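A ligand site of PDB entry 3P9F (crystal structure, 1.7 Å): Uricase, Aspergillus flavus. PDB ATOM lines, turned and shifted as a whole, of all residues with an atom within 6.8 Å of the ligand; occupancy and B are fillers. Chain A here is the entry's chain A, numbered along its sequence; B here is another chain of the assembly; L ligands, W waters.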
ATOM      1  N   SER A 158     -19.576 -35.315 -20.823  1.00  0.00           N
ATOM      2  CA  SER A 158     -20.282 -34.459 -19.885  1.00  0.00           C
ATOM      3  C   SER A 158     -21.765 -34.863 -19.957  1.00  0.00           C
ATOM      4  O   SER A 158     -22.255 -35.057 -21.056  1.00  0.00           O
ATOM      5  CB  SER A 158     -20.139 -32.968 -20.175  1.00  0.00           C
ATOM      6  OG  SER A 158     -20.925 -32.149 -19.348  1.00  0.00           O
ATOM      7  N   GLN A 159     -22.388 -35.008 -18.800  1.00  0.00           N
ATOM      8  CA  GLN A 159     -23.783 -35.379 -18.688  1.00  0.00           C
ATOM      9  C   GLN A 159     -24.503 -34.490 -17.702  1.00  0.00           C
ATOM     10  O   GLN A 159     -23.892 -33.857 -16.844  1.00  0.00           O
ATOM     11  CB  GLN A 159     -23.878 -36.861 -18.277  1.00  0.00           C
ATOM     12  CG  GLN A 159     -22.978 -37.786 -19.075  1.00  0.00           C
ATOM     13  CD  GLN A 159     -23.144 -39.229 -18.620  1.00  0.00           C
ATOM     14  OE1 GLN A 159     -24.249 -39.664 -18.305  1.00  0.00           O
ATOM     15  NE2 GLN A 159     -22.038 -39.962 -18.581  1.00  0.00           N
ATOM     16  N   PHE A 160     -25.833 -34.458 -17.815  1.00  0.00           N
ATOM     17  CA  PHE A 160     -26.653 -33.800 -16.804  1.00  0.00           C
ATOM     18  C   PHE A 160     -28.073 -34.372 -16.900  1.00  0.00           C
ATOM     19  O   PHE A 160     -28.849 -34.010 -17.780  1.00  0.00           O
ATOM     20  CB  PHE A 160     -26.654 -32.269 -16.945  1.00  0.00           C
ATOM     21  CG  PHE A 160     -27.246 -31.583 -15.725  1.00  0.00           C
ATOM     22  CD1 PHE A 160     -26.644 -31.804 -14.477  1.00  0.00           C
ATOM     23  CD2 PHE A 160     -28.340 -30.768 -15.804  1.00  0.00           C
ATOM     24  CE1 PHE A 160     -27.206 -31.193 -13.375  1.00  0.00           C
ATOM     25  CE2 PHE A 160     -28.917 -30.157 -14.694  1.00  0.00           C
ATOM     26  CZ  PHE A 160     -28.321 -30.371 -13.445  1.00  0.00           C
ATOM     27  N   PHE A 163     -31.899 -34.358 -12.464  1.00  0.00           N
ATOM     28  CA  PHE A 163     -32.179 -33.158 -11.703  1.00  0.00           C
ATOM     29  C   PHE A 163     -33.675 -33.025 -11.406  1.00  0.00           C
ATOM     30  O   PHE A 163     -34.508 -33.713 -12.002  1.00  0.00           O
ATOM     31  CB  PHE A 163     -31.695 -31.884 -12.411  1.00  0.00           C
ATOM     32  CG  PHE A 163     -32.063 -31.851 -13.896  1.00  0.00           C
ATOM     33  CD1 PHE A 163     -31.259 -32.480 -14.840  1.00  0.00           C
ATOM     34  CD2 PHE A 163     -33.212 -31.171 -14.254  1.00  0.00           C
ATOM     35  CE1 PHE A 163     -31.628 -32.415 -16.192  1.00  0.00           C
ATOM     36  CE2 PHE A 163     -33.573 -31.088 -15.591  1.00  0.00           C
ATOM     37  CZ  PHE A 163     -32.772 -31.722 -16.515  1.00  0.00           C
ATOM     38  N   LEU A 171     -35.856 -28.074 -19.275  1.00  0.00           N
ATOM     39  CA  LEU A 171     -34.598 -28.660 -19.721  1.00  0.00           C
ATOM     40  C   LEU A 171     -34.664 -30.156 -19.921  1.00  0.00           C
ATOM     41  O   LEU A 171     -35.048 -30.903 -19.019  1.00  0.00           O
ATOM     42  CB  LEU A 171     -33.508 -28.335 -18.687  1.00  0.00           C
ATOM     43  CG  LEU A 171     -32.118 -28.877 -18.952  1.00  0.00           C
ATOM     44  CD1 LEU A 171     -31.514 -28.211 -20.190  1.00  0.00           C
ATOM     45  CD2 LEU A 171     -31.208 -28.635 -17.762  1.00  0.00           C
ATOM     46  N   ARG A 177     -23.199 -34.056 -23.622  1.00  0.00           N
ATOM     47  CA  ARG A 177     -23.312 -32.645 -23.940  1.00  0.00           C
ATOM     48  C   ARG A 177     -21.895 -32.070 -23.968  1.00  0.00           C
ATOM     49  O   ARG A 177     -20.940 -32.736 -23.567  1.00  0.00           O
ATOM     50  CB  ARG A 177     -24.155 -31.874 -22.934  1.00  0.00           C
ATOM     51  CG  ARG A 177     -23.534 -31.945 -21.534  1.00  0.00           C
ATOM     52  CD  ARG A 177     -24.373 -31.100 -20.562  1.00  0.00           C
ATOM     53  NE  ARG A 177     -23.627 -30.938 -19.317  1.00  0.00           N
ATOM     54  CZ  ARG A 177     -23.986 -30.181 -18.312  1.00  0.00           C
ATOM     55  NH1 ARG A 177     -25.112 -29.458 -18.304  1.00  0.00           N
ATOM     56  NH2 ARG A 177     -23.207 -30.123 -17.245  1.00  0.00           N
ATOM     57  N   LEU A 179     -19.235 -29.402 -22.426  1.00  0.00           N
ATOM     58  CA  LEU A 179     -19.017 -28.617 -21.192  1.00  0.00           C
ATOM     59  C   LEU A 179     -17.858 -27.646 -21.442  1.00  0.00           C
ATOM     60  O   LEU A 179     -16.772 -28.113 -21.806  1.00  0.00           O
ATOM     61  CB  LEU A 179     -18.684 -29.513 -20.017  1.00  0.00           C
ATOM     62  CG  LEU A 179     -18.368 -28.834 -18.664  1.00  0.00           C
ATOM     63  CD1 LEU A 179     -19.493 -27.942 -18.200  1.00  0.00           C
ATOM     64  CD2 LEU A 179     -18.045 -29.927 -17.632  1.00  0.00           C
ATOM     65  N   SER A 225     -18.280 -36.357 -16.538  1.00  0.00           N
ATOM     66  CA  SER A 225     -18.935 -35.485 -15.590  1.00  0.00           C
ATOM     67  C   SER A 225     -20.428 -35.685 -15.427  1.00  0.00           C
ATOM     68  O   SER A 225     -21.212 -35.646 -16.387  1.00  0.00           O
ATOM     69  CB  SER A 225     -18.669 -34.018 -16.006  1.00  0.00           C
ATOM     70  OG  SER A 225     -19.413 -33.117 -15.227  1.00  0.00           O
ATOM     71  N   ALA A 226     -20.849 -35.857 -14.180  1.00  0.00           N
ATOM     72  CA  ALA A 226     -22.262 -35.954 -13.817  1.00  0.00           C
ATOM     73  C   ALA A 226     -22.935 -34.605 -13.696  1.00  0.00           C
ATOM     74  O   ALA A 226     -24.139 -34.480 -13.730  1.00  0.00           O
ATOM     75  CB  ALA A 226     -22.376 -36.709 -12.492  1.00  0.00           C
ATOM     76  N   SER A 227     -22.092 -33.574 -13.501  1.00  0.00           N
ATOM     77  CA  SER A 227     -22.478 -32.197 -13.361  1.00  0.00           C
ATOM     78  C   SER A 227     -21.224 -31.341 -13.111  1.00  0.00           C
ATOM     79  O   SER A 227     -20.188 -31.913 -12.791  1.00  0.00           O
ATOM     80  CB  SER A 227     -23.480 -31.921 -12.227  1.00  0.00           C
ATOM     81  OG  SER A 227     -22.861 -32.245 -10.982  1.00  0.00           O
ATOM     82  N   VAL A 228     -21.379 -30.031 -13.251  1.00  0.00           N
ATOM     83  CA  VAL A 228     -20.279 -29.124 -12.892  1.00  0.00           C
ATOM     84  C   VAL A 228     -19.978 -29.304 -11.409  1.00  0.00           C
ATOM     85  O   VAL A 228     -18.816 -29.391 -10.997  1.00  0.00           O
ATOM     86  CB  VAL A 228     -20.643 -27.682 -13.241  1.00  0.00           C
ATOM     87  CG1 VAL A 228     -19.585 -26.713 -12.736  1.00  0.00           C
ATOM     88  CG2 VAL A 228     -20.793 -27.515 -14.751  1.00  0.00           C
ATOM     89  N   GLN A 229     -21.039 -29.368 -10.614  1.00  0.00           N
ATOM     90  CA  GLN A 229     -20.876 -29.528  -9.163  1.00  0.00           C
ATOM     91  C   GLN A 229     -19.974 -30.691  -8.808  1.00  0.00           C
ATOM     92  O   GLN A 229     -19.004 -30.624  -8.038  1.00  0.00           O
ATOM     93  CB  GLN A 229     -22.268 -29.684  -8.553  1.00  0.00           C
ATOM     94  CG  GLN A 229     -23.156 -28.466  -8.499  1.00  0.00           C
ATOM     95  CD  GLN A 229     -24.034 -28.268  -9.732  1.00  0.00           C
ATOM     96  OE1 GLN A 229     -23.671 -28.679 -10.828  1.00  0.00           O
ATOM     97  NE2 GLN A 229     -25.169 -27.616  -9.474  1.00  0.00           N
ATOM     98  N   ASN A 255     -21.136 -22.217 -16.428  1.00  0.00           N
ATOM     99  CA  ASN A 255     -21.426 -23.226 -17.446  1.00  0.00           C
ATOM    100  C   ASN A 255     -21.742 -22.457 -18.733  1.00  0.00           C
ATOM    101  O   ASN A 255     -22.812 -21.882 -18.827  1.00  0.00           O
ATOM    102  CB  ASN A 255     -22.598 -24.082 -16.982  1.00  0.00           C
ATOM    103  CG  ASN A 255     -22.741 -25.371 -17.762  1.00  0.00           C
ATOM    104  OD1 ASN A 255     -22.134 -25.545 -18.813  1.00  0.00           O
ATOM    105  ND2 ASN A 255     -23.558 -26.299 -17.286  1.00  0.00           N
ATOM    106  N   HIS A 257     -22.934 -22.306 -22.013  1.00  0.00           N
ATOM    107  CA  HIS A 257     -23.744 -23.282 -22.750  1.00  0.00           C
ATOM    108  C   HIS A 257     -23.533 -23.270 -24.267  1.00  0.00           C
ATOM    109  O   HIS A 257     -23.403 -22.193 -24.857  1.00  0.00           O
ATOM    110  CB  HIS A 257     -25.226 -23.042 -22.477  1.00  0.00           C
ATOM    111  CG  HIS A 257     -25.589 -22.986 -21.023  1.00  0.00           C
ATOM    112  ND1 HIS A 257     -25.425 -24.053 -20.179  1.00  0.00           N
ATOM    113  CD2 HIS A 257     -26.081 -21.972 -20.291  1.00  0.00           C
ATOM    114  CE1 HIS A 257     -25.825 -23.691 -18.965  1.00  0.00           C
ATOM    115  NE2 HIS A 257     -26.230 -22.436 -19.002  1.00  0.00           N
ATOM    116  N   GLY A 287     -25.049 -20.702 -16.523  1.00  0.00           N
ATOM    117  CA  GLY A 287     -25.042 -21.242 -15.163  1.00  0.00           C
ATOM    118  C   GLY A 287     -23.824 -20.700 -14.424  1.00  0.00           C
ATOM    119  O   GLY A 287     -22.797 -20.430 -15.038  1.00  0.00           O
ATOM    120  N   ILE A 289     -21.726 -21.864 -10.885  1.00  0.00           N
ATOM    121  CA  ILE A 289     -21.656 -22.942  -9.879  1.00  0.00           C
ATOM    122  C   ILE A 289     -20.499 -22.653  -8.929  1.00  0.00           C
ATOM    123  O   ILE A 289     -19.386 -22.474  -9.421  1.00  0.00           O
ATOM    124  CB  ILE A 289     -21.515 -24.297 -10.559  1.00  0.00           C
ATOM    125  CG1 ILE A 289     -22.475 -24.476 -11.749  1.00  0.00           C
ATOM    126  CG2 ILE A 289     -21.673 -25.436  -9.552  1.00  0.00           C
ATOM    127  CD1 ILE A 289     -23.936 -24.352 -11.378  1.00  0.00           C
ATOM    128  N   TYR B   9     -25.342 -21.939  -6.178  1.00  0.00           N
ATOM    129  CA  TYR B   9     -25.296 -22.195  -7.624  1.00  0.00           C
ATOM    130  C   TYR B   9     -26.551 -21.556  -8.212  1.00  0.00           C
ATOM    131  O   TYR B   9     -27.550 -21.341  -7.527  1.00  0.00           O
ATOM    132  CB  TYR B   9     -25.141 -23.702  -7.916  1.00  0.00           C
ATOM    133  CG  TYR B   9     -26.540 -24.292  -7.951  1.00  0.00           C
ATOM    134  CD1 TYR B   9     -27.173 -24.470  -6.721  1.00  0.00           C
ATOM    135  CD2 TYR B   9     -27.193 -24.606  -9.150  1.00  0.00           C
ATOM    136  CE1 TYR B   9     -28.440 -24.993  -6.632  1.00  0.00           C
ATOM    137  CE2 TYR B   9     -28.500 -25.100  -9.048  1.00  0.00           C
ATOM    138  CZ  TYR B   9     -29.092 -25.283  -7.814  1.00  0.00           C
ATOM    139  OH  TYR B   9     -30.382 -25.783  -7.753  1.00  0.00           O
ATOM    140  N   GLY B  10     -26.557 -21.285  -9.524  1.00  0.00           N
ATOM    141  CA  GLY B  10     -27.760 -20.792 -10.162  1.00  0.00           C
ATOM    142  C   GLY B  10     -27.453 -20.219 -11.560  1.00  0.00           C
ATOM    143  O   GLY B  10     -26.534 -20.731 -12.203  1.00  0.00           O
ATOM    144  N   LYS B  11     -28.221 -19.217 -11.940  1.00  0.00           N
ATOM    145  CA  LYS B  11     -28.055 -18.652 -13.285  1.00  0.00           C
ATOM    146  C   LYS B  11     -27.671 -17.189 -13.181  1.00  0.00           C
ATOM    147  O   LYS B  11     -28.305 -16.424 -12.453  1.00  0.00           O
ATOM    148  CB  LYS B  11     -29.344 -18.795 -14.099  1.00  0.00           C
ATOM    149  CG  LYS B  11     -29.174 -18.583 -15.613  1.00  0.00           C
ATOM    150  CD  LYS B  11     -28.442 -19.706 -16.293  1.00  0.00           C
ATOM    151  CE  LYS B  11     -29.342 -20.696 -17.002  1.00  0.00           C
ATOM    152  NZ  LYS B  11     -28.616 -21.949 -17.373  1.00  0.00           N
ATOM    153  N   ASN B  52     -28.016 -35.457  -8.415  1.00  0.00           N
ATOM    154  CA  ASN B  52     -28.648 -34.283  -8.996  1.00  0.00           C
ATOM    155  C   ASN B  52     -30.091 -34.054  -8.607  1.00  0.00           C
ATOM    156  O   ASN B  52     -30.698 -33.040  -8.945  1.00  0.00           O
ATOM    157  CB  ASN B  52     -28.546 -34.372 -10.540  1.00  0.00           C
ATOM    158  CG  ASN B  52     -27.123 -34.158 -11.019  1.00  0.00           C
ATOM    159  OD1 ASN B  52     -26.323 -33.510 -10.343  1.00  0.00           O
ATOM    160  ND2 ASN B  52     -26.810 -34.692 -12.192  1.00  0.00           N
ATOM    161  N   ILE B  55     -30.896 -30.790  -7.191  1.00  0.00           N
ATOM    162  CA  ILE B  55     -30.661 -29.591  -8.008  1.00  0.00           C
ATOM    163  C   ILE B  55     -31.906 -29.105  -8.746  1.00  0.00           C
ATOM    164  O   ILE B  55     -32.441 -29.893  -9.540  1.00  0.00           O
ATOM    165  CB  ILE B  55     -29.527 -29.825  -9.035  1.00  0.00           C
ATOM    166  CG1 ILE B  55     -28.189 -30.204  -8.405  1.00  0.00           C
ATOM    167  CG2 ILE B  55     -29.409 -28.547  -9.888  1.00  0.00           C
ATOM    168  CD1 ILE B  55     -27.190 -30.738  -9.417  1.00  0.00           C
ATOM    169  N   VAL B  56     -32.250 -27.874  -8.451  1.00  0.00           N
ATOM    170  CA  VAL B  56     -33.229 -27.081  -9.228  1.00  0.00           C
ATOM    171  C   VAL B  56     -32.391 -26.580 -10.418  1.00  0.00           C
ATOM    172  O   VAL B  56     -31.492 -25.770 -10.178  1.00  0.00           O
ATOM    173  CB  VAL B  56     -33.868 -25.914  -8.495  1.00  0.00           C
ATOM    174  CG1 VAL B  56     -34.741 -25.062  -9.421  1.00  0.00           C
ATOM    175  CG2 VAL B  56     -34.719 -26.411  -7.316  1.00  0.00           C
ATOM    176  N   ALA B  57     -32.621 -27.078 -11.624  1.00  0.00           N
ATOM    177  CA  ALA B  57     -31.679 -26.780 -12.717  1.00  0.00           C
ATOM    178  C   ALA B  57     -31.547 -25.271 -12.931  1.00  0.00           C
ATOM    179  O   ALA B  57     -32.519 -24.520 -12.774  1.00  0.00           O
ATOM    180  CB  ALA B  57     -32.132 -27.469 -13.985  1.00  0.00           C
ATOM    181  N   THR B  58     -30.327 -24.853 -13.279  1.00  0.00           N
ATOM    182  CA  THR B  58     -30.158 -23.403 -13.504  1.00  0.00           C
ATOM    183  C   THR B  58     -31.073 -22.960 -14.650  1.00  0.00           C
ATOM    184  O   THR B  58     -31.548 -21.837 -14.634  1.00  0.00           O
ATOM    185  CB  THR B  58     -28.699 -23.020 -13.771  1.00  0.00           C
ATOM    186  OG1 THR B  58     -28.301 -23.572 -15.043  1.00  0.00           O
ATOM    187  CG2 THR B  58     -27.750 -23.628 -12.735  1.00  0.00           C
ATOM    188  N   ASP B  59     -31.298 -23.858 -15.612  1.00  0.00           N
ATOM    189  CA  ASP B  59     -32.210 -23.539 -16.705  1.00  0.00           C
ATOM    190  C   ASP B  59     -33.605 -23.265 -16.165  1.00  0.00           C
ATOM    191  O   ASP B  59     -34.338 -22.403 -16.637  1.00  0.00           O
ATOM    192  CB  ASP B  59     -32.268 -24.697 -17.711  1.00  0.00           C
ATOM    193  CG  ASP B  59     -33.084 -24.328 -18.947  1.00  0.00           C
ATOM    194  OD1 ASP B  59     -32.520 -23.618 -19.827  1.00  0.00           O
ATOM    195  OD2 ASP B  59     -34.265 -24.728 -19.025  1.00  0.00           O
ATOM    196  N   SER B  60     -34.004 -24.045 -15.128  1.00  0.00           N
ATOM    197  CA  SER B  60     -35.273 -23.787 -14.484  1.00  0.00           C
ATOM    198  C   SER B  60     -35.330 -22.494 -13.706  1.00  0.00           C
ATOM    199  O   SER B  60     -36.328 -21.791 -13.637  1.00  0.00           O
ATOM    200  CB  SER B  60     -35.618 -24.969 -13.530  1.00  0.00           C
ATOM    201  OG  SER B  60     -35.554 -26.182 -14.277  1.00  0.00           O
HETATM  202  N1  LIG L   1     -25.345 -28.165 -13.266  1.00  0.00           N
HETATM  203  C1  LIG L   1     -24.873 -28.595 -14.499  1.00  0.00           C
HETATM  204  O1  LIG L   1     -23.818 -29.173 -14.562  1.00  0.00           O
HETATM  205  N2  LIG L   1     -25.648 -28.344 -15.604  1.00  0.00           N
HETATM  206  C2  LIG L   1     -26.829 -27.709 -15.406  1.00  0.00           C
HETATM  207  C3  LIG L   1     -27.304 -27.295 -14.167  1.00  0.00           C
HETATM  208  C4  LIG L   1     -26.487 -27.497 -12.983  1.00  0.00           C
HETATM  209  O2  LIG L   1     -26.799 -27.169 -11.840  1.00  0.00           O
HETATM  210  N3  LIG L   1     -28.481 -26.717 -14.263  1.00  0.00           N
HETATM  211  N4  LIG L   1     -28.756 -26.739 -15.564  1.00  0.00           N
HETATM  212  N5  LIG L   1     -27.780 -27.331 -16.313  1.00  0.00           N
HETATM  213  O   HOH W   1     -27.479 -27.283 -19.148  1.00  0.00           O
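Water W1 bridges a nitrogen (N5) of the ligand (2.9 Å) and the guanidinium group (NH1) of Arg 177 (3.3 Å).
The backbone NH of Thr 58 of chain B lies within hydrogen-bond range of a nitrogen (N3) of the ligand. The side-chain hydroxyl of Thr 58 of chain B sits at hydrogen-bond distance from a nitrogen (N4) of the ligand. N of Val 228 lies within hydrogen-bond range of O1 of the ligand, 2.9 Å away. NE2 of Gln 229 sits at hydrogen-bond distance from O2 of the ligand (2.9 Å). NH2 of Arg 177 lies within hydrogen-bond range of O1 of the ligand (2.9 Å). The side-chain amide nitrogen (ND2) of Asn 255 sits close to a nitrogen (N2) of the ligand (3.4 Å).
Merely in contact with the ligand: Phe 160, Leu 171, Ser 227, Tyr 9 of chain B, Ile 55 of chain B, Ala 57 of chain B and Asp 59 of chain B. 12 residues have an atom within 4 Å of the ligand: Phe 160, Leu 171, Arg 177, Ser 227, Val 228, Gln 229, Asn 255, Tyr 9 of chain B, Ile 55 of chain B, Ala 57 of chain B, Thr 58 of chain B and Asp 59 of chain B. The nearest printed residue that does not touch the ligand is Ile 289 (4.04 Å).
The side-chain amino group of Lys 11 of chain B lies within hydrogen-bond range of the side-chain hydroxyl of Thr 58 of chain B, at 2.9 Å. The backbone NH (N) of Gln 229 lies close to the side-chain hydroxyl (OG) of Ser 227 (3.4 Å). The backbone NH (N) of Arg 177 is in hydrogen-bond range of the backbone carbonyl oxygen (O) of Ser 158 (2.9 Å). The backbone carbonyl oxygen (O) of Asn 255 lies within hydrogen-bond range of a ring nitrogen (NE2) of His 257. The backbone NH of Asn 255 is in hydrogen-bond range of the backbone carbonyl oxygen of Gly 287 (2.8 Å). O of Ser 227 is in hydrogen-bond range of OG of Ser 225. The side-chain hydroxyl (OH) of Tyr 9 of chain B sits at hydrogen-bond distance from the backbone carbonyl oxygen (O) of Val 56 of chain B.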
